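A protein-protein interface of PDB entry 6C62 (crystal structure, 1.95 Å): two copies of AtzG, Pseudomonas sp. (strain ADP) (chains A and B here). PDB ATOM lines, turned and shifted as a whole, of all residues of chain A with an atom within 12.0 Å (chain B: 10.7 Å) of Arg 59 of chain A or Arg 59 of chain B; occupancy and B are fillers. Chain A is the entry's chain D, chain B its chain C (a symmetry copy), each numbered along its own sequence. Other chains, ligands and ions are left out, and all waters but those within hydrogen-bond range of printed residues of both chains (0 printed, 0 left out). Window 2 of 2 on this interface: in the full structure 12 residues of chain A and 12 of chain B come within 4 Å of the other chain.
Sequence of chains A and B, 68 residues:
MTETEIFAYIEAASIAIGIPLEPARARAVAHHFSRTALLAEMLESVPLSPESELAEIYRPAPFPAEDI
The guanidinium group (NH1) of Arg 59 of chain B lies within salt-bridge range of the side-chain carboxylate (OE1) of Glu 56 of chain B (3.2 Å). The guanidinium group of Arg 59 of chain B lies within hydrogen-bond range of the backbone carbonyl oxygen of Ile 57 of chain B (3.5 Å).
Of the 12 printed residues of chain A, 4 touch a printed residue of chain B. Of the 10 printed residues of chain B, 4 touch a printed residue of chain A. Along chain B the printed residues that touch a printed residue of chain A span positions 56 to 59. Among the printed residues, 8 pairs touch across the chains.
Of chain B, only Glu 56 (3.1 Å) and Arg 59 (3.1 Å) come within 4 Å of Arg 59 of chain A. Printed residues of chain A within 4 Å of Arg 59 of chain B: Glu 56 and Arg 59. Tyr 58 of chain A touches one residue of chain B. No residue of chain B comes within 4 Å of Pro 60 of chain A. No residue of chain B comes within 4 Å of Ala 61 of chain A. Glu 56 of chain B touches just these residues of chain A: Glu 56, Ile 57, Tyr 58 and Arg 59. Tyr 58 of chain B touches one residue of chain A. No residue of chain A comes within 4 Å of Pro 60 of chain B. No residue of chain A comes within 4 Å of Ala 61 of chain B. No residue of chain A comes within 4 Å of Pro 62 of chain B. Of the printed residues of chain B, Ile 57 of chain A touches Glu 56. Printed residues of chain A within 4 Å of Ile 57 of chain B: Glu 56 (3.7 Å). Printed residues of chain B within 4 Å of Glu 56 of chain A: Glu 56, Ile 57, Tyr 58 and Arg 59.
The side-chain carboxylate of Glu 56 of chain A lies within salt-bridge range of the guanidinium group of Arg 59 of chain B, at 2.6 Å. The side-chain carboxylate (OE2) of Glu 56 of chain B lies within hydrogen-bond range of the backbone NH (N) of Arg 59 of chain A. The guanidinium group (NE) of Arg 59 of chain A lies close to the guanidinium group (NH2) of Arg 59 of chain B, 3.1 Å away.
Glu 56 of chain B touches its own counterpart, Glu 56 of chain A. Glu 56 of chain A touches Ile 57 of chain B, and with the chains exchanged Ile 57 of chain A touches Glu 56 of chain B. Glu 56 of chain A touches Arg 59 of chain B, and with the chains exchanged Arg 59 of chain A touches Glu 56 of chain B. Arg 59 of chain B touches its own counterpart, Arg 59 of chain A. Positions printed for both chains: 54, 55, 56, 57, 58, 59, 60, 61, 62 and 63. Of the 8 pairs that touch across the chains among the printed residues, 8 have their exchanged pair printed and touching as well.
Glu 56 of chain B touches Glu 56 of chain A (CB to CB, 3.7 Å). Ile 57 of chain B touches Glu 56 of chain A (O to CG, 3.7 Å). Tyr 58 of chain B touches Glu 56 of chain A (CA to CG, 3.6 Å). Ile 57 of chain A touches Glu 56 of chain B. CA of Tyr 58 of chain A touches CG of Glu 56 of chain B, 3.6 Å away.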
ATOM      1  N   GLU A  53     -22.147  -3.781 -16.299  1.00  0.00           N
ATOM      2  CA  GLU A  53     -22.303  -4.007 -17.726  1.00  0.00           C
ATOM      3  C   GLU A  53     -21.427  -3.098 -18.620  1.00  0.00           C
ATOM      4  O   GLU A  53     -20.935  -2.062 -18.210  1.00  0.00           O
ATOM      5  CB  GLU A  53     -23.798  -3.852 -18.090  1.00  0.00           C
ATOM      6  CG  GLU A  53     -24.691  -4.777 -17.267  1.00  0.00           C
ATOM      7  CD  GLU A  53     -26.006  -5.177 -17.933  1.00  0.00           C
ATOM      8  OE1 GLU A  53     -26.229  -4.931 -19.129  1.00  0.00           O
ATOM      9  OE2 GLU A  53     -26.828  -5.767 -17.222  1.00  0.00           O
ATOM     10  N   LEU A  54     -21.347  -3.488 -19.884  1.00  0.00           N
ATOM     11  CA  LEU A  54     -20.796  -2.671 -20.932  1.00  0.00           C
ATOM     12  C   LEU A  54     -21.492  -1.310 -20.978  1.00  0.00           C
ATOM     13  O   LEU A  54     -22.679  -1.185 -20.654  1.00  0.00           O
ATOM     14  CB  LEU A  54     -21.001  -3.365 -22.298  1.00  0.00           C
ATOM     15  CG  LEU A  54     -20.326  -4.731 -22.543  1.00  0.00           C
ATOM     16  CD1 LEU A  54     -20.912  -5.426 -23.759  1.00  0.00           C
ATOM     17  CD2 LEU A  54     -18.768  -4.661 -22.621  1.00  0.00           C
ATOM     18  N   ALA A  55     -20.725  -0.308 -21.380  1.00  0.00           N
ATOM     19  CA  ALA A  55     -21.239   1.046 -21.488  1.00  0.00           C
ATOM     20  C   ALA A  55     -22.412   1.152 -22.500  1.00  0.00           C
ATOM     21  O   ALA A  55     -23.338   1.933 -22.270  1.00  0.00           O
ATOM     22  CB  ALA A  55     -20.107   2.031 -21.835  1.00  0.00           C
ATOM     23  N   GLU A  56     -22.415   0.335 -23.531  1.00  0.00           N
ATOM     24  CA  GLU A  56     -23.544   0.325 -24.484  1.00  0.00           C
ATOM     25  C   GLU A  56     -24.035  -1.092 -24.779  1.00  0.00           C
ATOM     26  O   GLU A  56     -23.266  -2.012 -25.084  1.00  0.00           O
ATOM     27  CB  GLU A  56     -23.177   1.027 -25.791  1.00  0.00           C
ATOM     28  CG  GLU A  56     -22.807   2.524 -25.593  1.00  0.00           C
ATOM     29  CD  GLU A  56     -23.959   3.359 -25.015  1.00  0.00           C
ATOM     30  OE1 GLU A  56     -25.119   3.065 -25.275  1.00  0.00           O
ATOM     31  OE2 GLU A  56     -23.754   4.291 -24.267  1.00  0.00           O
ATOM     32  N   ILE A  57     -25.337  -1.259 -24.650  1.00  0.00           N
ATOM     33  CA  ILE A  57     -25.950  -2.586 -24.780  1.00  0.00           C
ATOM     34  C   ILE A  57     -26.839  -2.479 -26.060  1.00  0.00           C
ATOM     35  O   ILE A  57     -27.522  -1.479 -26.297  1.00  0.00           O
ATOM     36  CB  ILE A  57     -26.814  -2.868 -23.527  1.00  0.00           C
ATOM     37  CG1 ILE A  57     -25.979  -2.828 -22.244  1.00  0.00           C
ATOM     38  CG2 ILE A  57     -27.571  -4.176 -23.655  1.00  0.00           C
ATOM     39  CD1 ILE A  57     -24.856  -3.824 -22.240  1.00  0.00           C
ATOM     40  N   TYR A  58     -26.877  -3.549 -26.811  1.00  0.00           N
ATOM     41  CA  TYR A  58     -27.672  -3.668 -28.052  1.00  0.00           C
ATOM     42  C   TYR A  58     -29.127  -3.224 -27.956  1.00  0.00           C
ATOM     43  O   TYR A  58     -29.809  -3.452 -26.949  1.00  0.00           O
ATOM     44  CB  TYR A  58     -27.632  -5.127 -28.432  1.00  0.00           C
ATOM     45  CG  TYR A  58     -28.225  -5.466 -29.747  1.00  0.00           C
ATOM     46  CD1 TYR A  58     -27.622  -5.060 -30.892  1.00  0.00           C
ATOM     47  CD2 TYR A  58     -29.365  -6.244 -29.842  1.00  0.00           C
ATOM     48  CE1 TYR A  58     -28.132  -5.401 -32.105  1.00  0.00           C
ATOM     49  CE2 TYR A  58     -29.894  -6.581 -31.088  1.00  0.00           C
ATOM     50  CZ  TYR A  58     -29.253  -6.179 -32.193  1.00  0.00           C
ATOM     51  OH  TYR A  58     -29.727  -6.419 -33.408  1.00  0.00           O
ATOM     52  N   ARG A  59     -29.588  -2.590 -29.002  1.00  0.00           N
ATOM     53  CA  ARG A  59     -31.001  -2.190 -29.156  1.00  0.00           C
ATOM     54  C   ARG A  59     -31.413  -2.799 -30.518  1.00  0.00           C
ATOM     55  O   ARG A  59     -30.815  -2.473 -31.573  1.00  0.00           O
ATOM     56  CB  ARG A  59     -31.113  -0.675 -29.207  1.00  0.00           C
ATOM     57  CG  ARG A  59     -30.652   0.012 -27.904  1.00  0.00           C
ATOM     58  CD  ARG A  59     -30.263   1.436 -28.177  1.00  0.00           C
ATOM     59  NE  ARG A  59     -29.994   2.200 -26.950  1.00  0.00           N
ATOM     60  CZ  ARG A  59     -30.892   2.926 -26.268  1.00  0.00           C
ATOM     61  NH1 ARG A  59     -32.198   2.974 -26.611  1.00  0.00           N
ATOM     62  NH2 ARG A  59     -30.477   3.599 -25.191  1.00  0.00           N
ATOM     63  N   PRO A  60     -32.373  -3.729 -30.498  1.00  0.00           N
ATOM     64  CA  PRO A  60     -32.685  -4.446 -31.727  1.00  0.00           C
ATOM     65  C   PRO A  60     -33.457  -3.623 -32.786  1.00  0.00           C
ATOM     66  O   PRO A  60     -33.416  -3.999 -33.961  1.00  0.00           O
ATOM     67  CB  PRO A  60     -33.515  -5.627 -31.245  1.00  0.00           C
ATOM     68  CG  PRO A  60     -34.212  -5.059 -29.999  1.00  0.00           C
ATOM     69  CD  PRO A  60     -33.188  -4.178 -29.366  1.00  0.00           C
ATOM     70  N   ALA A  61     -34.154  -2.598 -32.344  1.00  0.00           N
ATOM     71  CA  ALA A  61     -34.922  -1.640 -33.175  1.00  0.00           C
ATOM     72  C   ALA A  61     -35.464  -0.551 -32.262  1.00  0.00           C
ATOM     73  O   ALA A  61     -35.628  -0.763 -31.055  1.00  0.00           O
ATOM     74  CB  ALA A  61     -36.106  -2.340 -33.927  1.00  0.00           C
ATOM     75  N   PRO A  62     -35.828   0.597 -32.830  1.00  0.00           N
ATOM     76  CA  PRO A  62     -36.405   1.665 -31.941  1.00  0.00           C
ATOM     77  C   PRO A  62     -37.713   1.168 -31.379  1.00  0.00           C
ATOM     78  O   PRO A  62     -38.434   0.416 -32.035  1.00  0.00           O
ATOM     79  CB  PRO A  62     -36.647   2.861 -32.885  1.00  0.00           C
ATOM     80  CG  PRO A  62     -35.788   2.532 -34.104  1.00  0.00           C
ATOM     81  CD  PRO A  62     -35.697   1.043 -34.231  1.00  0.00           C
ATOM     82  N   PHE A  63     -37.998   1.567 -30.163  1.00  0.00           N
ATOM     83  CA  PHE A  63     -39.219   1.163 -29.500  1.00  0.00           C
ATOM     84  C   PHE A  63     -40.363   1.923 -30.150  1.00  0.00           C
ATOM     85  O   PHE A  63     -40.250   3.121 -30.304  1.00  0.00           O
ATOM     86  CB  PHE A  63     -39.132   1.426 -27.970  1.00  0.00           C
ATOM     87  CG  PHE A  63     -40.254   0.772 -27.212  1.00  0.00           C
ATOM     88  CD1 PHE A  63     -40.253  -0.584 -26.941  1.00  0.00           C
ATOM     89  CD2 PHE A  63     -41.391   1.518 -26.859  1.00  0.00           C
ATOM     90  CE1 PHE A  63     -41.316  -1.169 -26.263  1.00  0.00           C
ATOM     91  CE2 PHE A  63     -42.457   0.919 -26.232  1.00  0.00           C
ATOM     92  CZ  PHE A  63     -42.421  -0.424 -25.931  1.00  0.00           C
ATOM     93  N   PRO A  64     -41.457   1.251 -30.540  1.00  0.00           N
ATOM     94  CA  PRO A  64     -42.457   1.972 -31.371  1.00  0.00           C
ATOM     95  C   PRO A  64     -43.221   3.047 -30.571  1.00  0.00           C
ATOM     96  O   PRO A  64     -43.496   2.856 -29.376  1.00  0.00           O
ATOM     97  CB  PRO A  64     -43.387   0.854 -31.843  1.00  0.00           C
ATOM     98  CG  PRO A  64     -43.297  -0.187 -30.791  1.00  0.00           C
ATOM     99  CD  PRO A  64     -41.888  -0.121 -30.236  1.00  0.00           C
ATOM    100  N   LEU B  54     -19.742  -0.170 -35.375  1.00  0.00           N
ATOM    101  CA  LEU B  54     -20.256  -1.008 -34.290  1.00  0.00           C
ATOM    102  C   LEU B  54     -21.784  -0.834 -34.162  1.00  0.00           C
ATOM    103  O   LEU B  54     -22.314   0.239 -34.394  1.00  0.00           O
ATOM    104  CB  LEU B  54     -19.590  -0.627 -32.974  1.00  0.00           C
ATOM    105  CG  LEU B  54     -18.055  -0.759 -32.866  1.00  0.00           C
ATOM    106  CD1 LEU B  54     -17.525   0.015 -31.670  1.00  0.00           C
ATOM    107  CD2 LEU B  54     -17.545  -2.215 -32.813  1.00  0.00           C
ATOM    108  N   ALA B  55     -22.445  -1.921 -33.785  1.00  0.00           N
ATOM    109  CA  ALA B  55     -23.857  -1.948 -33.543  1.00  0.00           C
ATOM    110  C   ALA B  55     -24.278  -0.948 -32.467  1.00  0.00           C
ATOM    111  O   ALA B  55     -25.351  -0.373 -32.587  1.00  0.00           O
ATOM    112  CB  ALA B  55     -24.315  -3.383 -33.202  1.00  0.00           C
ATOM    113  N   GLU B  56     -23.436  -0.678 -31.469  1.00  0.00           N
ATOM    114  CA  GLU B  56     -23.768   0.338 -30.467  1.00  0.00           C
ATOM    115  C   GLU B  56     -22.632   1.323 -30.239  1.00  0.00           C
ATOM    116  O   GLU B  56     -21.464   0.950 -29.960  1.00  0.00           O
ATOM    117  CB  GLU B  56     -24.187  -0.330 -29.134  1.00  0.00           C
ATOM    118  CG  GLU B  56     -25.470  -1.148 -29.267  1.00  0.00           C
ATOM    119  CD  GLU B  56     -26.708  -0.337 -29.752  1.00  0.00           C
ATOM    120  OE1 GLU B  56     -26.819   0.837 -29.448  1.00  0.00           O
ATOM    121  OE2 GLU B  56     -27.577  -0.832 -30.488  1.00  0.00           O
ATOM    122  N   ILE B  57     -22.980   2.587 -30.334  1.00  0.00           N
ATOM    123  CA  ILE B  57     -22.011   3.645 -30.202  1.00  0.00           C
ATOM    124  C   ILE B  57     -22.322   4.396 -28.885  1.00  0.00           C
ATOM    125  O   ILE B  57     -23.479   4.640 -28.563  1.00  0.00           O
ATOM    126  CB  ILE B  57     -22.099   4.601 -31.433  1.00  0.00           C
ATOM    127  CG1 ILE B  57     -21.907   3.853 -32.764  1.00  0.00           C
ATOM    128  CG2 ILE B  57     -21.114   5.752 -31.294  1.00  0.00           C
ATOM    129  CD1 ILE B  57     -20.541   3.157 -32.825  1.00  0.00           C
ATOM    130  N   TYR B  58     -21.274   4.766 -28.169  1.00  0.00           N
ATOM    131  CA  TYR B  58     -21.331   5.520 -26.922  1.00  0.00           C
ATOM    132  C   TYR B  58     -22.283   6.707 -26.875  1.00  0.00           C
ATOM    133  O   TYR B  58     -22.397   7.461 -27.815  1.00  0.00           O
ATOM    134  CB  TYR B  58     -19.950   5.962 -26.574  1.00  0.00           C
ATOM    135  CG  TYR B  58     -19.789   6.582 -25.213  1.00  0.00           C
ATOM    136  CD1 TYR B  58     -19.883   5.809 -24.083  1.00  0.00           C
ATOM    137  CD2 TYR B  58     -19.450   7.889 -25.071  1.00  0.00           C
ATOM    138  CE1 TYR B  58     -19.688   6.326 -22.846  1.00  0.00           C
ATOM    139  CE2 TYR B  58     -19.255   8.440 -23.807  1.00  0.00           C
ATOM    140  CZ  TYR B  58     -19.345   7.658 -22.722  1.00  0.00           C
ATOM    141  OH  TYR B  58     -19.217   8.212 -21.498  1.00  0.00           O
ATOM    142  N   ARG B  59     -22.992   6.824 -25.764  1.00  0.00           N
ATOM    143  CA  ARG B  59     -23.882   7.955 -25.475  1.00  0.00           C
ATOM    144  C   ARG B  59     -23.353   8.520 -24.155  1.00  0.00           C
ATOM    145  O   ARG B  59     -23.357   7.834 -23.140  1.00  0.00           O
ATOM    146  CB  ARG B  59     -25.315   7.481 -25.350  1.00  0.00           C
ATOM    147  CG  ARG B  59     -25.863   6.793 -26.620  1.00  0.00           C
ATOM    148  CD  ARG B  59     -27.046   5.951 -26.265  1.00  0.00           C
ATOM    149  NE  ARG B  59     -27.723   5.361 -27.424  1.00  0.00           N
ATOM    150  CZ  ARG B  59     -27.475   4.160 -27.953  1.00  0.00           C
ATOM    151  NH1 ARG B  59     -26.519   3.359 -27.477  1.00  0.00           N
ATOM    152  NH2 ARG B  59     -28.195   3.755 -29.002  1.00  0.00           N
ATOM    153  N   PRO B  60     -22.846   9.766 -24.174  1.00  0.00           N
ATOM    154  CA  PRO B  60     -22.195  10.274 -22.971  1.00  0.00           C
ATOM    155  C   PRO B  60     -23.179  10.653 -21.832  1.00  0.00           C
ATOM    156  O   PRO B  60     -22.766  10.697 -20.671  1.00  0.00           O
ATOM    157  CB  PRO B  60     -21.429  11.480 -23.485  1.00  0.00           C
ATOM    158  CG  PRO B  60     -22.257  11.969 -24.657  1.00  0.00           C
ATOM    159  CD  PRO B  60     -22.824  10.729 -25.295  1.00  0.00           C
ATOM    160  N   ALA B  61     -24.418  10.982 -22.191  1.00  0.00           N
ATOM    161  CA  ALA B  61     -25.481  11.379 -21.268  1.00  0.00           C
ATOM    162  C   ALA B  61     -26.757  11.536 -22.125  1.00  0.00           C
ATOM    163  O   ALA B  61     -26.677  11.811 -23.340  1.00  0.00           O
ATOM    164  CB  ALA B  61     -25.195  12.689 -20.515  1.00  0.00           C
ATOM    165  N   PRO B  62     -27.943  11.420 -21.493  1.00  0.00           N
ATOM    166  CA  PRO B  62     -29.168  11.669 -22.278  1.00  0.00           C
ATOM    167  C   PRO B  62     -29.188  13.086 -22.817  1.00  0.00           C
ATOM    168  O   PRO B  62     -28.689  14.007 -22.181  1.00  0.00           O
ATOM    169  CB  PRO B  62     -30.307  11.451 -21.279  1.00  0.00           C
ATOM    170  CG  PRO B  62     -29.675  11.099 -19.972  1.00  0.00           C
ATOM    171  CD  PRO B  62     -28.205  11.146 -20.075  1.00  0.00           C
ATOM    172  N   PHE B  63     -29.731  13.242 -24.002  1.00  0.00           N
ATOM    173  CA  PHE B  63     -29.867  14.573 -24.581  1.00  0.00           C
ATOM    174  C   PHE B  63     -30.971  15.328 -23.788  1.00  0.00           C
ATOM    175  O   PHE B  63     -32.031  14.771 -23.573  1.00  0.00           O
ATOM    176  CB  PHE B  63     -30.202  14.451 -26.062  1.00  0.00           C
ATOM    177  CG  PHE B  63     -30.093  15.766 -26.788  1.00  0.00           C
ATOM    178  CD1 PHE B  63     -28.832  16.279 -27.150  1.00  0.00           C
ATOM    179  CD2 PHE B  63     -31.228  16.548 -27.029  1.00  0.00           C
ATOM    180  CE1 PHE B  63     -28.735  17.484 -27.804  1.00  0.00           C
ATOM    181  CE2 PHE B  63     -31.113  17.779 -27.617  1.00  0.00           C
ATOM    182  CZ  PHE B  63     -29.861  18.255 -27.992  1.00  0.00           C
